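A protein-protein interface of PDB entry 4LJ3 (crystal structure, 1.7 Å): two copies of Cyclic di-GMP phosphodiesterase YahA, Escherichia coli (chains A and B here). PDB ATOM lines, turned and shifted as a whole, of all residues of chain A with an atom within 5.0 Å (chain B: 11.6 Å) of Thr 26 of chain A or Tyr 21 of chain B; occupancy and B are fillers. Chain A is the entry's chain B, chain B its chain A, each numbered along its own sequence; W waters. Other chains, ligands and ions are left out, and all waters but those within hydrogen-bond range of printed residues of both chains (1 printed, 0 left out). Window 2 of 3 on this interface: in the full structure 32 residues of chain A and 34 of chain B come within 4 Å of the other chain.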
ATOM      1  N   ILE A  24       0.228 -15.994  26.743  1.00  0.00           N
ATOM      2  CA  ILE A  24       0.044 -14.650  27.310  1.00  0.00           C
ATOM      3  C   ILE A  24      -1.353 -14.616  27.911  1.00  0.00           C
ATOM      4  O   ILE A  24      -2.366 -14.541  27.200  1.00  0.00           O
ATOM      5  CB  ILE A  24       0.215 -13.549  26.248  1.00  0.00           C
ATOM      6  CG1 ILE A  24       1.609 -13.651  25.629  1.00  0.00           C
ATOM      7  CG2 ILE A  24       0.008 -12.166  26.865  1.00  0.00           C
ATOM      8  CD1 ILE A  24       1.763 -12.901  24.331  1.00  0.00           C
ATOM      9  N   VAL A  25      -1.380 -14.628  29.235  1.00  0.00           N
ATOM     10  CA  VAL A  25      -2.487 -15.186  29.999  1.00  0.00           C
ATOM     11  C   VAL A  25      -2.960 -14.036  30.882  1.00  0.00           C
ATOM     12  O   VAL A  25      -2.164 -13.140  31.147  1.00  0.00           O
ATOM     13  CB  VAL A  25      -1.921 -16.399  30.789  1.00  0.00           C
ATOM     14  CG1 VAL A  25      -2.433 -16.535  32.220  1.00  0.00           C
ATOM     15  CG2 VAL A  25      -2.113 -17.691  30.001  1.00  0.00           C
ATOM     16  N   THR A  26      -4.229 -14.037  31.304  1.00  0.00           N
ATOM     17  CA  THR A  26      -4.785 -12.985  32.160  1.00  0.00           C
ATOM     18  C   THR A  26      -5.243 -13.592  33.480  1.00  0.00           C
ATOM     19  O   THR A  26      -5.386 -14.815  33.587  1.00  0.00           O
ATOM     20  CB  THR A  26      -6.019 -12.347  31.499  1.00  0.00           C
ATOM     21  OG1 THR A  26      -7.016 -13.362  31.328  1.00  0.00           O
ATOM     22  CG2 THR A  26      -5.664 -11.743  30.159  1.00  0.00           C
ATOM     23  N   PRO A  27      -5.503 -12.745  34.489  1.00  0.00           N
ATOM     24  CA  PRO A  27      -6.060 -13.264  35.734  1.00  0.00           C
ATOM     25  C   PRO A  27      -7.335 -14.074  35.523  1.00  0.00           C
ATOM     26  O   PRO A  27      -7.538 -15.089  36.189  1.00  0.00           O
ATOM     27  CB  PRO A  27      -6.347 -11.992  36.545  1.00  0.00           C
ATOM     28  CG  PRO A  27      -5.319 -11.022  36.064  1.00  0.00           C
ATOM     29  CD  PRO A  27      -5.188 -11.304  34.591  1.00  0.00           C
ATOM     30  N   GLU A  28      -8.169 -13.644  34.572  1.00  0.00           N
ATOM     31  CA  GLU A  28      -9.413 -14.334  34.254  1.00  0.00           C
ATOM     32  C   GLU A  28      -9.154 -15.744  33.714  1.00  0.00           C
ATOM     33  O   GLU A  28      -9.901 -16.669  34.016  1.00  0.00           O
ATOM     34  CB  GLU A  28     -10.226 -13.533  33.226  1.00  0.00           C
ATOM     35  CG  GLU A  28     -10.853 -12.250  33.758  1.00  0.00           C
ATOM     36  CD  GLU A  28      -9.946 -11.028  33.602  1.00  0.00           C
ATOM     37  OE1 GLU A  28      -8.718 -11.127  33.808  1.00  0.00           O
ATOM     38  OE2 GLU A  28     -10.447  -9.941  33.255  1.00  0.00           O
ATOM     39  N   ALA A  29      -8.097 -15.906  32.924  1.00  0.00           N
ATOM     40  CA  ALA A  29      -7.729 -17.222  32.406  1.00  0.00           C
ATOM     41  C   ALA A  29      -7.233 -18.152  33.526  1.00  0.00           C
ATOM     42  O   ALA A  29      -7.591 -19.315  33.561  1.00  0.00           O
ATOM     43  CB  ALA A  29      -6.679 -17.090  31.322  1.00  0.00           C
ATOM     44  N   ILE A  30      -6.416 -17.629  34.433  1.00  0.00           N
ATOM     45  CA  ILE A  30      -5.903 -18.424  35.556  1.00  0.00           C
ATOM     46  C   ILE A  30      -7.064 -18.830  36.460  1.00  0.00           C
ATOM     47  O   ILE A  30      -7.189 -19.995  36.836  1.00  0.00           O
ATOM     48  CB  ILE A  30      -4.823 -17.655  36.351  1.00  0.00           C
ATOM     49  CG1 ILE A  30      -3.586 -17.429  35.482  1.00  0.00           C
ATOM     50  CG2 ILE A  30      -4.443 -18.411  37.626  1.00  0.00           C
ATOM     51  CD1 ILE A  30      -2.625 -16.381  36.011  1.00  0.00           C
ATOM     52  N   LEU A  79       2.244 -13.871  37.123  1.00  0.00           N
ATOM     53  CA  LEU A  79       0.919 -13.255  37.142  1.00  0.00           C
ATOM     54  C   LEU A  79       0.072 -13.813  38.269  1.00  0.00           C
ATOM     55  O   LEU A  79      -0.708 -13.086  38.870  1.00  0.00           O
ATOM     56  CB  LEU A  79       0.199 -13.448  35.790  1.00  0.00           C
ATOM     57  CG  LEU A  79      -1.186 -12.813  35.624  1.00  0.00           C
ATOM     58  CD1 LEU A  79      -1.163 -11.318  35.901  1.00  0.00           C
ATOM     59  CD2 LEU A  79      -1.717 -13.082  34.226  1.00  0.00           C
ATOM     60  N   TYR B  21      -8.335 -12.962  28.813  1.00  0.00           N
ATOM     61  CA  TYR B  21      -8.052 -13.775  27.591  1.00  0.00           C
ATOM     62  C   TYR B  21      -6.764 -14.602  27.675  1.00  0.00           C
ATOM     63  O   TYR B  21      -5.949 -14.486  28.599  1.00  0.00           O
ATOM     64  CB  TYR B  21      -8.056 -12.884  26.325  1.00  0.00           C
ATOM     65  CG  TYR B  21      -8.194 -13.657  25.027  1.00  0.00           C
ATOM     66  CD1 TYR B  21      -9.401 -14.246  24.658  1.00  0.00           C
ATOM     67  CD2 TYR B  21      -7.102 -13.828  24.182  1.00  0.00           C
ATOM     68  CE1 TYR B  21      -9.516 -14.973  23.481  1.00  0.00           C
ATOM     69  CE2 TYR B  21      -7.208 -14.550  23.009  1.00  0.00           C
ATOM     70  CZ  TYR B  21      -8.414 -15.118  22.659  1.00  0.00           C
ATOM     71  OH  TYR B  21      -8.506 -15.828  21.482  1.00  0.00           O
ATOM     72  N   HIS B  22      -6.622 -15.478  26.693  1.00  0.00           N
ATOM     73  CA  HIS B  22      -5.489 -16.369  26.578  1.00  0.00           C
ATOM     74  C   HIS B  22      -4.963 -16.284  25.140  1.00  0.00           C
ATOM     75  O   HIS B  22      -5.538 -16.874  24.208  1.00  0.00           O
ATOM     76  CB  HIS B  22      -5.966 -17.778  26.927  1.00  0.00           C
ATOM     77  CG  HIS B  22      -4.873 -18.789  27.036  1.00  0.00           C
ATOM     78  ND1 HIS B  22      -4.952 -19.856  27.901  1.00  0.00           N
ATOM     79  CD2 HIS B  22      -3.684 -18.907  26.400  1.00  0.00           C
ATOM     80  CE1 HIS B  22      -3.864 -20.593  27.788  1.00  0.00           C
ATOM     81  NE2 HIS B  22      -3.081 -20.040  26.883  1.00  0.00           N
ATOM     82  N   HIS B  23      -3.894 -15.512  24.954  1.00  0.00           N
ATOM     83  CA  HIS B  23      -3.250 -15.422  23.643  1.00  0.00           C
ATOM     84  C   HIS B  23      -2.085 -16.406  23.617  1.00  0.00           C
ATOM     85  O   HIS B  23      -1.334 -16.502  24.593  1.00  0.00           O
ATOM     86  CB  HIS B  23      -2.756 -14.002  23.329  1.00  0.00           C
ATOM     87  CG  HIS B  23      -3.810 -13.112  22.755  1.00  0.00           C
ATOM     88  ND1 HIS B  23      -4.472 -13.422  21.587  1.00  0.00           N
ATOM     89  CD2 HIS B  23      -4.315 -11.925  23.170  1.00  0.00           C
ATOM     90  CE1 HIS B  23      -5.342 -12.469  21.307  1.00  0.00           C
ATOM     91  NE2 HIS B  23      -5.272 -11.552  22.256  1.00  0.00           N
ATOM     92  N   ILE B  24      -1.969 -17.145  22.515  1.00  0.00           N
ATOM     93  CA  ILE B  24      -0.891 -18.115  22.314  1.00  0.00           C
ATOM     94  C   ILE B  24       0.089 -17.652  21.231  1.00  0.00           C
ATOM     95  O   ILE B  24      -0.288 -17.533  20.059  1.00  0.00           O
ATOM     96  CB  ILE B  24      -1.436 -19.495  21.889  1.00  0.00           C
ATOM     97  CG1 ILE B  24      -2.408 -20.033  22.944  1.00  0.00           C
ATOM     98  CG2 ILE B  24      -0.293 -20.486  21.681  1.00  0.00           C
ATOM     99  CD1 ILE B  24      -3.288 -21.163  22.458  1.00  0.00           C
ATOM    100  N   VAL B  25       1.346 -17.440  21.625  1.00  0.00           N
ATOM    101  CA  VAL B  25       2.419 -17.156  20.664  1.00  0.00           C
ATOM    102  C   VAL B  25       3.052 -18.403  20.058  1.00  0.00           C
ATOM    103  O   VAL B  25       3.683 -19.237  20.725  1.00  0.00           O
ATOM    104  CB  VAL B  25       3.481 -16.164  21.181  1.00  0.00           C
ATOM    105  CG1 VAL B  25       4.438 -15.850  20.044  1.00  0.00           C
ATOM    106  CG2 VAL B  25       2.790 -14.907  21.690  1.00  0.00           C
ATOM    107  N   THR B  26       2.841 -18.486  18.752  1.00  0.00           N
ATOM    108  CA  THR B  26       3.336 -19.534  17.891  1.00  0.00           C
ATOM    109  C   THR B  26       4.241 -18.900  16.841  1.00  0.00           C
ATOM    110  O   THR B  26       4.214 -17.679  16.651  1.00  0.00           O
ATOM    111  CB  THR B  26       2.165 -20.211  17.139  1.00  0.00           C
ATOM    112  OG1 THR B  26       1.510 -19.237  16.316  1.00  0.00           O
ATOM    113  CG2 THR B  26       1.174 -20.807  18.117  1.00  0.00           C
ATOM    114  N   ALA B  29       2.277 -16.696  14.582  1.00  0.00           N
ATOM    115  CA  ALA B  29       1.955 -15.379  15.136  1.00  0.00           C
ATOM    116  C   ALA B  29       3.140 -14.407  15.027  1.00  0.00           C
ATOM    117  O   ALA B  29       2.957 -13.259  14.671  1.00  0.00           O
ATOM    118  CB  ALA B  29       1.515 -15.507  16.579  1.00  0.00           C
ATOM    119  N   HIS B  65       1.762  -4.875  19.631  1.00  0.00           N
ATOM    120  CA  HIS B  65       0.664  -5.595  18.990  1.00  0.00           C
ATOM    121  C   HIS B  65      -0.597  -4.726  19.062  1.00  0.00           C
ATOM    122  O   HIS B  65      -1.034  -4.384  20.159  1.00  0.00           O
ATOM    123  CB  HIS B  65       0.433  -6.922  19.702  1.00  0.00           C
ATOM    124  CG  HIS B  65      -0.562  -7.809  19.014  1.00  0.00           C
ATOM    125  ND1 HIS B  65      -0.223  -8.985  18.372  1.00  0.00           N
ATOM    126  CD2 HIS B  65      -1.900  -7.686  18.883  1.00  0.00           C
ATOM    127  CE1 HIS B  65      -1.313  -9.530  17.858  1.00  0.00           C
ATOM    128  NE2 HIS B  65      -2.342  -8.765  18.160  1.00  0.00           N
ATOM    129  N   GLN B  67      -3.849  -4.872  18.887  1.00  0.00           N
ATOM    130  CA  GLN B  67      -4.995  -5.206  19.742  1.00  0.00           C
ATOM    131  C   GLN B  67      -4.691  -5.382  21.229  1.00  0.00           C
ATOM    132  O   GLN B  67      -5.569  -5.145  22.059  1.00  0.00           O
ATOM    133  CB  GLN B  67      -5.707  -6.459  19.224  1.00  0.00           C
ATOM    134  CG  GLN B  67      -6.628  -6.189  18.042  1.00  0.00           C
ATOM    135  CD  GLN B  67      -7.710  -7.247  17.876  1.00  0.00           C
ATOM    136  OE1 GLN B  67      -7.730  -8.255  18.579  1.00  0.00           O
ATOM    137  NE2 GLN B  67      -8.622  -7.013  16.941  1.00  0.00           N
ATOM    138  N   THR B  68      -3.477  -5.805  21.573  1.00  0.00           N
ATOM    139  CA  THR B  68      -3.152  -6.145  22.964  1.00  0.00           C
ATOM    140  C   THR B  68      -2.101  -5.261  23.635  1.00  0.00           C
ATOM    141  O   THR B  68      -1.860  -5.414  24.835  1.00  0.00           O
ATOM    142  CB  THR B  68      -2.651  -7.597  23.075  1.00  0.00           C
ATOM    143  OG1 THR B  68      -1.552  -7.781  22.178  1.00  0.00           O
ATOM    144  CG2 THR B  68      -3.746  -8.571  22.724  1.00  0.00           C
ATOM    145  N   GLY B  69      -1.481  -4.349  22.889  1.00  0.00           N
ATOM    146  CA  GLY B  69      -0.498  -3.445  23.463  1.00  0.00           C
ATOM    147  C   GLY B  69       0.908  -4.025  23.405  1.00  0.00           C
ATOM    148  O   GLY B  69       1.207  -4.868  22.551  1.00  0.00           O
ATOM    149  N   ILE B  71       4.092  -6.145  24.238  1.00  0.00           N
ATOM    150  CA  ILE B  71       4.478  -7.448  24.756  1.00  0.00           C
ATOM    151  C   ILE B  71       6.007  -7.472  24.945  1.00  0.00           C
ATOM    152  O   ILE B  71       6.746  -7.191  23.994  1.00  0.00           O
ATOM    153  CB  ILE B  71       4.020  -8.555  23.783  1.00  0.00           C
ATOM    154  CG1 ILE B  71       2.500  -8.485  23.566  1.00  0.00           C
ATOM    155  CG2 ILE B  71       4.430  -9.936  24.281  1.00  0.00           C
ATOM    156  CD1 ILE B  71       1.991  -9.359  22.435  1.00  0.00           C
ATOM    157  N   GLN B  75       8.263 -13.016  26.587  1.00  0.00           N
ATOM    158  CA  GLN B  75       7.081 -13.714  26.063  1.00  0.00           C
ATOM    159  C   GLN B  75       7.119 -14.024  24.553  1.00  0.00           C
ATOM    160  O   GLN B  75       6.074 -14.373  23.963  1.00  0.00           O
ATOM    161  CB  GLN B  75       5.834 -12.913  26.400  1.00  0.00           C
ATOM    162  CG  GLN B  75       5.655 -12.660  27.887  1.00  0.00           C
ATOM    163  CD  GLN B  75       4.258 -12.165  28.231  1.00  0.00           C
ATOM    164  OE1 GLN B  75       3.638 -12.640  29.186  1.00  0.00           O
ATOM    165  NE2 GLN B  75       3.744 -11.248  27.446  1.00  0.00           N
HETATM  166  O   HOH W   1      -4.156 -12.113  27.039  1.00  0.00           O
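The backbone carbonyl oxygen (O) of His 23 of chain B is in hydrogen-bond range of the backbone NH (N) of Ile 24 of chain A (2.7 Å). The backbone NH (N) of Tyr 21 of chain B is in hydrogen-bond range of the side-chain hydroxyl (OG1) of Thr 26 of chain A (2.9 Å).
The backbone NH (N) of Glu 28 of chain A lies close to the side-chain hydroxyl (OG1) of Thr 26 of chain A, at 3.5 Å. The side-chain hydroxyl (OG1) of Thr 26 of chain A is in hydrogen-bond range of the backbone NH (N) of Ala 29 of chain A.
Tyr 21 of chain B touches Ile 24 of chain A (O to O, 3.8 Å). Ile 24 of chain A touches His 22 of chain B. Val 25 of chain B touches Ile 24 of chain A (CG2 to CD1, 3.5 Å). CG2 of Ile 71 of chain B touches CD1 of Ile 24 of chain A, 3.99 Å away. NE2 of Gln 75 of chain B touches CG1 of Ile 24 of chain A (3.7 Å). C of Val 25 of chain A touches O of Tyr 21 of chain B, 3.8 Å away. CB of Ala 29 of chain A touches O of Tyr 21 of chain B, 3.8 Å away.
Tyr 21 of chain B touches four residues of chain A. Val 25 of chain A touches just one residue of chain B: Tyr 21. No residue of chain B comes within 4 Å of Glu 28 of chain A. Of the printed residues of chain B, Ala 29 of chain A touches Tyr 21 (3.8 Å). Of the printed residues of chain A, His 22 of chain B touches Ile 24. Of the printed residues of chain A, Val 25 of chain B touches Ile 24 (3.5 Å). Printed residues of chain A within 4 Å of His 23 of chain B: Ile 24. The nearest residue of chain B that does not touch Thr 26 of chain A is His 22 of chain B (5.1 Å).
Of the 13 printed residues of chain B, 6 touch a printed residue of chain A. Hydrophobic or aromatic side chains of chain B that line the printed part of chain A: His 23, Val 25 and Ile 71. Along chain B the printed residues that touch a printed residue of chain A span positions 21 to 75. Printed residues of chain A that touch a printed residue of chain B: Ile 24, Val 25, Thr 26 and Ala 29. Among the printed residues, no Asp or Glu carboxylate lies within 4 Å of a Lys or Arg side-chain nitrogen of the other chain.
Ile 24 of chain A touches Val 25 of chain B, but with the chains exchanged Val 25 of chain A does not touch Ile 24 of chain B (7.2 Å). 4 positions are printed for both chains. Of the 9 pairs that touch across the chains among the printed residues, none has its exchanged pair printed and touching as well.
Water W1 bridges the backbone carbonyl oxygen (O) of Ile 24 of chain A and the backbone carbonyl oxygen (O) of Tyr 21 of chain B.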
